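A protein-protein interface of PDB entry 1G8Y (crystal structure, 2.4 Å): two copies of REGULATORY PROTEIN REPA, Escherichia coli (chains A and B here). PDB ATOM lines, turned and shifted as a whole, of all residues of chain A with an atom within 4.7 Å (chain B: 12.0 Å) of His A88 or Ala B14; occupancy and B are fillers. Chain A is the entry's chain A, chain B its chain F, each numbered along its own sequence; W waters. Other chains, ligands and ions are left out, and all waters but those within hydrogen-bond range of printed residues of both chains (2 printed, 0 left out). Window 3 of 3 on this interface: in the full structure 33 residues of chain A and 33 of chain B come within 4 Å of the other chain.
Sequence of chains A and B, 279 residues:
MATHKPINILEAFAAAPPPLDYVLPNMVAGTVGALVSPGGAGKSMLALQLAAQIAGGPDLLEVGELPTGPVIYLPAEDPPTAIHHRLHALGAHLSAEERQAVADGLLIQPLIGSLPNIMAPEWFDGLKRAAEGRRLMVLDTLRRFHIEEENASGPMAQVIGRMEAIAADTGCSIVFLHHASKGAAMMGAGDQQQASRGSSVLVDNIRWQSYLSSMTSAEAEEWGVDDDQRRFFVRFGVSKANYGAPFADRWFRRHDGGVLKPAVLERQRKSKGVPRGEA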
ATOM      1  N   HIS A  84     -13.176   6.557 -34.036  1.00  0.00           N
ATOM      2  CA  HIS A  84     -13.223   7.322 -32.791  1.00  0.00           C
ATOM      3  C   HIS A  84     -14.064   6.570 -31.764  1.00  0.00           C
ATOM      4  O   HIS A  84     -13.671   6.460 -30.602  1.00  0.00           O
ATOM      5  CB  HIS A  84     -13.870   8.695 -33.024  1.00  0.00           C
ATOM      6  CG  HIS A  84     -13.076   9.603 -33.907  1.00  0.00           C
ATOM      7  ND1 HIS A  84     -13.669  10.540 -34.730  1.00  0.00           N
ATOM      8  CD2 HIS A  84     -11.740   9.721 -34.099  1.00  0.00           C
ATOM      9  CE1 HIS A  84     -12.732  11.194 -35.394  1.00  0.00           C
ATOM     10  NE2 HIS A  84     -11.554  10.715 -35.031  1.00  0.00           N
ATOM     11  N   HIS A  85     -15.233   6.084 -32.192  1.00  0.00           N
ATOM     12  CA  HIS A  85     -16.128   5.352 -31.300  1.00  0.00           C
ATOM     13  C   HIS A  85     -15.469   4.062 -30.834  1.00  0.00           C
ATOM     14  O   HIS A  85     -15.492   3.757 -29.638  1.00  0.00           O
ATOM     15  CB  HIS A  85     -17.482   5.061 -31.983  1.00  0.00           C
ATOM     16  CG  HIS A  85     -18.479   6.171 -31.835  1.00  0.00           C
ATOM     17  ND1 HIS A  85     -19.442   6.184 -30.848  1.00  0.00           N
ATOM     18  CD2 HIS A  85     -18.609   7.348 -32.501  1.00  0.00           C
ATOM     19  CE1 HIS A  85     -20.119   7.318 -30.909  1.00  0.00           C
ATOM     20  NE2 HIS A  85     -19.632   8.042 -31.903  1.00  0.00           N
ATOM     21  N   ARG A  86     -14.867   3.312 -31.753  1.00  0.00           N
ATOM     22  CA  ARG A  86     -14.206   2.087 -31.345  1.00  0.00           C
ATOM     23  C   ARG A  86     -13.094   2.368 -30.331  1.00  0.00           C
ATOM     24  O   ARG A  86     -12.909   1.605 -29.394  1.00  0.00           O
ATOM     25  CB  ARG A  86     -13.600   1.344 -32.542  1.00  0.00           C
ATOM     26  CG  ARG A  86     -14.579   0.639 -33.444  1.00  0.00           C
ATOM     27  CD  ARG A  86     -13.851  -0.494 -34.164  1.00  0.00           C
ATOM     28  NE  ARG A  86     -13.979  -0.408 -35.614  1.00  0.00           N
ATOM     29  CZ  ARG A  86     -15.085  -0.695 -36.286  1.00  0.00           C
ATOM     30  NH1 ARG A  86     -16.172  -1.098 -35.634  1.00  0.00           N
ATOM     31  NH2 ARG A  86     -15.110  -0.571 -37.609  1.00  0.00           N
ATOM     32  N   LEU A  87     -12.335   3.446 -30.525  1.00  0.00           N
ATOM     33  CA  LEU A  87     -11.248   3.774 -29.586  1.00  0.00           C
ATOM     34  C   LEU A  87     -11.775   4.199 -28.223  1.00  0.00           C
ATOM     35  O   LEU A  87     -11.217   3.833 -27.179  1.00  0.00           O
ATOM     36  CB  LEU A  87     -10.353   4.891 -30.141  1.00  0.00           C
ATOM     37  CG  LEU A  87      -9.308   4.421 -31.166  1.00  0.00           C
ATOM     38  CD1 LEU A  87      -8.737   5.636 -31.894  1.00  0.00           C
ATOM     39  CD2 LEU A  87      -8.214   3.586 -30.472  1.00  0.00           C
ATOM     40  N   HIS A  88     -12.853   4.974 -28.234  1.00  0.00           N
ATOM     41  CA  HIS A  88     -13.424   5.428 -26.986  1.00  0.00           C
ATOM     42  C   HIS A  88     -13.912   4.237 -26.174  1.00  0.00           C
ATOM     43  O   HIS A  88     -13.686   4.173 -24.960  1.00  0.00           O
ATOM     44  CB  HIS A  88     -14.584   6.381 -27.229  1.00  0.00           C
ATOM     45  CG  HIS A  88     -15.107   6.992 -25.973  1.00  0.00           C
ATOM     46  ND1 HIS A  88     -14.457   8.021 -25.326  1.00  0.00           N
ATOM     47  CD2 HIS A  88     -16.172   6.672 -25.202  1.00  0.00           C
ATOM     48  CE1 HIS A  88     -15.099   8.310 -24.209  1.00  0.00           C
ATOM     49  NE2 HIS A  88     -16.143   7.507 -24.109  1.00  0.00           N
ATOM     50  N   ALA A  89     -14.579   3.296 -26.845  1.00  0.00           N
ATOM     51  CA  ALA A  89     -15.094   2.106 -26.170  1.00  0.00           C
ATOM     52  C   ALA A  89     -13.952   1.263 -25.603  1.00  0.00           C
ATOM     53  O   ALA A  89     -13.992   0.844 -24.449  1.00  0.00           O
ATOM     54  CB  ALA A  89     -15.938   1.265 -27.123  1.00  0.00           C
ATOM     55  N   LEU A  90     -12.938   1.012 -26.416  1.00  0.00           N
ATOM     56  CA  LEU A  90     -11.809   0.217 -25.972  1.00  0.00           C
ATOM     57  C   LEU A  90     -11.122   0.898 -24.790  1.00  0.00           C
ATOM     58  O   LEU A  90     -10.669   0.235 -23.856  1.00  0.00           O
ATOM     59  CB  LEU A  90     -10.808   0.064 -27.100  1.00  0.00           C
ATOM     60  CG  LEU A  90      -9.468  -0.515 -26.686  1.00  0.00           C
ATOM     61  CD1 LEU A  90      -9.583  -2.035 -26.542  1.00  0.00           C
ATOM     62  CD2 LEU A  90      -8.431  -0.156 -27.748  1.00  0.00           C
ATOM     63  N   GLY A  91     -11.061   2.227 -24.843  1.00  0.00           N
ATOM     64  CA  GLY A  91     -10.406   2.996 -23.803  1.00  0.00           C
ATOM     65  C   GLY A  91     -10.972   2.844 -22.403  1.00  0.00           C
ATOM     66  O   GLY A  91     -10.261   3.014 -21.409  1.00  0.00           O
ATOM     67  N   ALA A  92     -12.254   2.520 -22.311  1.00  0.00           N
ATOM     68  CA  ALA A  92     -12.873   2.358 -21.011  1.00  0.00           C
ATOM     69  C   ALA A  92     -12.356   1.097 -20.327  1.00  0.00           C
ATOM     70  O   ALA A  92     -12.617   0.891 -19.141  1.00  0.00           O
ATOM     71  CB  ALA A  92     -14.386   2.305 -21.156  1.00  0.00           C
ATOM     72  N   ILE B   7      -5.541   9.808 -36.649  1.00  0.00           N
ATOM     73  CA  ILE B   7      -6.494   9.836 -35.552  1.00  0.00           C
ATOM     74  C   ILE B   7      -5.791  10.324 -34.293  1.00  0.00           C
ATOM     75  O   ILE B   7      -4.715   9.851 -33.970  1.00  0.00           O
ATOM     76  CB  ILE B   7      -7.014   8.408 -35.210  1.00  0.00           C
ATOM     77  CG1 ILE B   7      -7.798   7.829 -36.372  1.00  0.00           C
ATOM     78  CG2 ILE B   7      -7.910   8.463 -33.980  1.00  0.00           C
ATOM     79  CD1 ILE B   7      -9.054   8.537 -36.624  1.00  0.00           C
ATOM     80  N   ASN B   8      -6.393  11.259 -33.580  1.00  0.00           N
ATOM     81  CA  ASN B   8      -5.815  11.710 -32.327  1.00  0.00           C
ATOM     82  C   ASN B   8      -6.341  10.688 -31.310  1.00  0.00           C
ATOM     83  O   ASN B   8      -7.497  10.770 -30.852  1.00  0.00           O
ATOM     84  CB  ASN B   8      -6.328  13.104 -31.958  1.00  0.00           C
ATOM     85  CG  ASN B   8      -5.653  13.650 -30.710  1.00  0.00           C
ATOM     86  OD1 ASN B   8      -5.495  12.949 -29.704  1.00  0.00           O
ATOM     87  ND2 ASN B   8      -5.245  14.900 -30.773  1.00  0.00           N
ATOM     88  N   ILE B   9      -5.493   9.740 -30.939  1.00  0.00           N
ATOM     89  CA  ILE B   9      -5.908   8.684 -30.033  1.00  0.00           C
ATOM     90  C   ILE B   9      -6.303   9.070 -28.619  1.00  0.00           C
ATOM     91  O   ILE B   9      -7.291   8.556 -28.083  1.00  0.00           O
ATOM     92  CB  ILE B   9      -4.842   7.576 -30.002  1.00  0.00           C
ATOM     93  CG1 ILE B   9      -4.826   6.890 -31.381  1.00  0.00           C
ATOM     94  CG2 ILE B   9      -5.138   6.580 -28.851  1.00  0.00           C
ATOM     95  CD1 ILE B   9      -3.720   5.866 -31.593  1.00  0.00           C
ATOM     96  N   LEU B  10      -5.532   9.963 -28.017  1.00  0.00           N
ATOM     97  CA  LEU B  10      -5.789  10.423 -26.662  1.00  0.00           C
ATOM     98  C   LEU B  10      -7.123  11.202 -26.632  1.00  0.00           C
ATOM     99  O   LEU B  10      -7.952  11.054 -25.709  1.00  0.00           O
ATOM    100  CB  LEU B  10      -4.623  11.318 -26.226  1.00  0.00           C
ATOM    101  CG  LEU B  10      -3.683  10.826 -25.115  1.00  0.00           C
ATOM    102  CD1 LEU B  10      -3.748   9.304 -24.929  1.00  0.00           C
ATOM    103  CD2 LEU B  10      -2.284  11.287 -25.438  1.00  0.00           C
ATOM    104  N   GLU B  11      -7.333  12.029 -27.650  1.00  0.00           N
ATOM    105  CA  GLU B  11      -8.564  12.796 -27.714  1.00  0.00           C
ATOM    106  C   GLU B  11      -9.758  11.828 -27.897  1.00  0.00           C
ATOM    107  O   GLU B  11     -10.842  12.056 -27.363  1.00  0.00           O
ATOM    108  CB  GLU B  11      -8.449  13.837 -28.844  1.00  0.00           C
ATOM    109  CG  GLU B  11      -9.740  14.493 -29.314  1.00  0.00           C
ATOM    110  CD  GLU B  11     -10.321  15.489 -28.314  1.00  0.00           C
ATOM    111  OE1 GLU B  11     -11.320  16.159 -28.668  1.00  0.00           O
ATOM    112  OE2 GLU B  11      -9.783  15.603 -27.184  1.00  0.00           O
ATOM    113  N   ALA B  12      -9.559  10.727 -28.615  1.00  0.00           N
ATOM    114  CA  ALA B  12     -10.654   9.775 -28.813  1.00  0.00           C
ATOM    115  C   ALA B  12     -10.970   9.026 -27.535  1.00  0.00           C
ATOM    116  O   ALA B  12     -12.119   8.629 -27.325  1.00  0.00           O
ATOM    117  CB  ALA B  12     -10.316   8.787 -29.907  1.00  0.00           C
ATOM    118  N   PHE B  13      -9.946   8.817 -26.696  1.00  0.00           N
ATOM    119  CA  PHE B  13     -10.107   8.108 -25.423  1.00  0.00           C
ATOM    120  C   PHE B  13     -10.878   8.955 -24.419  1.00  0.00           C
ATOM    121  O   PHE B  13     -11.775   8.466 -23.731  1.00  0.00           O
ATOM    122  CB  PHE B  13      -8.736   7.760 -24.816  1.00  0.00           C
ATOM    123  CG  PHE B  13      -8.092   6.502 -25.387  1.00  0.00           C
ATOM    124  CD1 PHE B  13      -6.708   6.317 -25.289  1.00  0.00           C
ATOM    125  CD2 PHE B  13      -8.863   5.510 -25.989  1.00  0.00           C
ATOM    126  CE1 PHE B  13      -6.099   5.175 -25.781  1.00  0.00           C
ATOM    127  CE2 PHE B  13      -8.277   4.354 -26.486  1.00  0.00           C
ATOM    128  CZ  PHE B  13      -6.883   4.175 -26.387  1.00  0.00           C
ATOM    129  N   ALA B  14     -10.521  10.238 -24.367  1.00  0.00           N
ATOM    130  CA  ALA B  14     -11.109  11.205 -23.438  1.00  0.00           C
ATOM    131  C   ALA B  14     -12.558  11.570 -23.703  1.00  0.00           C
ATOM    132  O   ALA B  14     -13.469  11.072 -23.044  1.00  0.00           O
ATOM    133  CB  ALA B  14     -10.263  12.472 -23.422  1.00  0.00           C
ATOM    134  N   ALA B  15     -12.764  12.453 -24.664  1.00  0.00           N
ATOM    135  CA  ALA B  15     -14.111  12.903 -25.008  1.00  0.00           C
ATOM    136  C   ALA B  15     -15.036  11.800 -25.512  1.00  0.00           C
ATOM    137  O   ALA B  15     -14.675  11.080 -26.436  1.00  0.00           O
ATOM    138  CB  ALA B  15     -14.027  14.010 -26.065  1.00  0.00           C
ATOM    139  N   ALA B  16     -16.210  11.648 -24.894  1.00  0.00           N
ATOM    140  CA  ALA B  16     -17.183  10.670 -25.379  1.00  0.00           C
ATOM    141  C   ALA B  16     -17.526  11.296 -26.732  1.00  0.00           C
ATOM    142  O   ALA B  16     -17.953  12.454 -26.814  1.00  0.00           O
ATOM    143  CB  ALA B  16     -18.416  10.617 -24.479  1.00  0.00           C
ATOM    144  N   PRO B  17     -17.324  10.545 -27.815  1.00  0.00           N
ATOM    145  CA  PRO B  17     -17.610  11.094 -29.142  1.00  0.00           C
ATOM    146  C   PRO B  17     -19.062  11.438 -29.413  1.00  0.00           C
ATOM    147  O   PRO B  17     -19.981  10.892 -28.788  1.00  0.00           O
ATOM    148  CB  PRO B  17     -17.090  10.008 -30.092  1.00  0.00           C
ATOM    149  CG  PRO B  17     -16.055   9.247 -29.232  1.00  0.00           C
ATOM    150  CD  PRO B  17     -16.769   9.184 -27.909  1.00  0.00           C
ATOM    151  N   PRO B  18     -19.282  12.362 -30.354  1.00  0.00           N
ATOM    152  CA  PRO B  18     -20.627  12.787 -30.729  1.00  0.00           C
ATOM    153  C   PRO B  18     -21.381  11.545 -31.196  1.00  0.00           C
ATOM    154  O   PRO B  18     -20.779  10.588 -31.689  1.00  0.00           O
ATOM    155  CB  PRO B  18     -20.363  13.754 -31.881  1.00  0.00           C
ATOM    156  CG  PRO B  18     -19.026  14.322 -31.543  1.00  0.00           C
ATOM    157  CD  PRO B  18     -18.272  13.092 -31.137  1.00  0.00           C
ATOM    158  N   PRO B  19     -22.702  11.525 -31.022  1.00  0.00           N
ATOM    159  CA  PRO B  19     -23.389  10.316 -31.495  1.00  0.00           C
ATOM    160  C   PRO B  19     -23.074  10.096 -32.994  1.00  0.00           C
ATOM    161  O   PRO B  19     -22.838  11.052 -33.744  1.00  0.00           O
ATOM    162  CB  PRO B  19     -24.864  10.632 -31.247  1.00  0.00           C
ATOM    163  CG  PRO B  19     -24.818  11.578 -30.076  1.00  0.00           C
ATOM    164  CD  PRO B  19     -23.631  12.472 -30.383  1.00  0.00           C
ATOM    165  N   LEU B  20     -23.033   8.839 -33.416  1.00  0.00           N
ATOM    166  CA  LEU B  20     -22.760   8.524 -34.809  1.00  0.00           C
ATOM    167  C   LEU B  20     -23.932   9.090 -35.625  1.00  0.00           C
ATOM    168  O   LEU B  20     -25.097   8.919 -35.247  1.00  0.00           O
ATOM    169  CB  LEU B  20     -22.642   6.998 -34.976  1.00  0.00           C
ATOM    170  CG  LEU B  20     -21.344   6.400 -35.528  1.00  0.00           C
ATOM    171  CD1 LEU B  20     -20.150   7.352 -35.321  1.00  0.00           C
ATOM    172  CD2 LEU B  20     -21.113   5.047 -34.864  1.00  0.00           C
ATOM    173  N   TYR B 243     -22.856  -0.725 -37.361  1.00  0.00           N
ATOM    174  CA  TYR B 243     -23.135   0.113 -36.201  1.00  0.00           C
ATOM    175  C   TYR B 243     -24.621   0.287 -35.951  1.00  0.00           C
ATOM    176  O   TYR B 243     -25.434   0.156 -36.868  1.00  0.00           O
ATOM    177  CB  TYR B 243     -22.505   1.493 -36.398  1.00  0.00           C
ATOM    178  CG  TYR B 243     -21.210   1.447 -37.166  1.00  0.00           C
ATOM    179  CD1 TYR B 243     -19.986   1.288 -36.513  1.00  0.00           C
ATOM    180  CD2 TYR B 243     -21.215   1.513 -38.556  1.00  0.00           C
ATOM    181  CE1 TYR B 243     -18.802   1.187 -37.230  1.00  0.00           C
ATOM    182  CE2 TYR B 243     -20.044   1.415 -39.283  1.00  0.00           C
ATOM    183  CZ  TYR B 243     -18.842   1.254 -38.619  1.00  0.00           C
ATOM    184  OH  TYR B 243     -17.689   1.163 -39.367  1.00  0.00           O
HETATM  185  O   HOH W   1     -12.623   5.792 -22.781  1.00  0.00           O
HETATM  186  O   HOH W   2      -8.602  12.258 -34.460  1.00  0.00           O
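O of Ala B15 lies within hydrogen-bond range of ND1 of His A88, at 3.3 Å.
A ring nitrogen (ND1) of His A88 lies within hydrogen-bond range of the backbone carbonyl oxygen (O) of Phe B13 (3.2 Å).
ND1 of His A88 sits at hydrogen-bond distance from O of Ala B12 (3.1 Å).
O of Pro B18 is in hydrogen-bond range of NE2 of His A85.
Among the printed residues, pairs that only touch across the chains: His A84 with Ile B7 (3.7 Å), His A84 with Pro B17 (3.9 Å), His A85 with Pro B17 (3.7 Å), His A85 with Leu B20 (3.2 Å), Arg A86 with Tyr B243 (3.6 Å), Leu A87 with Ile B7 (3.6 Å), Leu A87 with Ala B12 (3.9 Å), Leu A87 with Phe B13 (3.1 Å), His A88 with Ala B14 (3.4 Å), His A88 with Ala B16 (3.4 Å), His A88 with Pro B17 (3.4 Å) and Gly A91 with Phe B13 (3.7 Å).
Of the printed residues of chain B, Arg A86 touches Tyr B243 (3.6 Å).
Printed residues of chain B within 4 Å of Leu A87: Ile B7, Ala B12 and Phe B13.
His A88 touches six residues of chain B.
No residue of chain B comes within 4 Å of Leu A90.
Asn B8 touches none of the printed residues of chain A.
Printed residues of chain A within 4 Å of Ala B12: Leu A87 (3.9 Å) and His A88 (3.1 Å).
Of the printed residues of chain A, Phe B13 touches Leu A87 (3.1 Å), His A88 (3.2 Å) and Gly A91 (3.7 Å).
Ala B14 touches just one residue of chain A: His A88.
Printed residues of chain A within 4 Å of Pro B17: His A84, His A85 and His A88.
Of the printed residues of chain A, Pro B18 touches His A85.
The nearest residue of chain B that does not touch His A88 is Glu B11 (5.8 Å).
The nearest printed residue of chain A that does not touch Ala B14 is Leu A87 (7.0 Å).
Printed residues of chain B that touch a printed residue of chain A: Ile B7, Ala B12, Phe B13, Ala B14, Ala B15, Ala B16, Pro B17, Pro B18, Leu B20 and Tyr B243.
Hydrophobic or aromatic side chains of chain A that line the printed part of chain B: His A84, His A85, Leu A87 and His A88.
Among the printed residues, 16 pairs touch across the chains.
Among the printed residues, no Asp or Glu carboxylate lies within 4 Å of a Lys or Arg side-chain nitrogen of the other chain.
No position is printed for both chains.
Of the 16 pairs that touch across the chains among the printed residues, none has its exchanged pair printed and touching as well.
Water W2 bridges the backbone NH (N) of Asn B8 (2.6 Å) and a ring nitrogen (NE2) of His A84 (3.4 Å).
Water W1 lies within hydrogen-bond range of O of His A88 (2.9 Å), O of Phe B13 (3.0 Å) and N of Ala A92 (3.3 Å).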
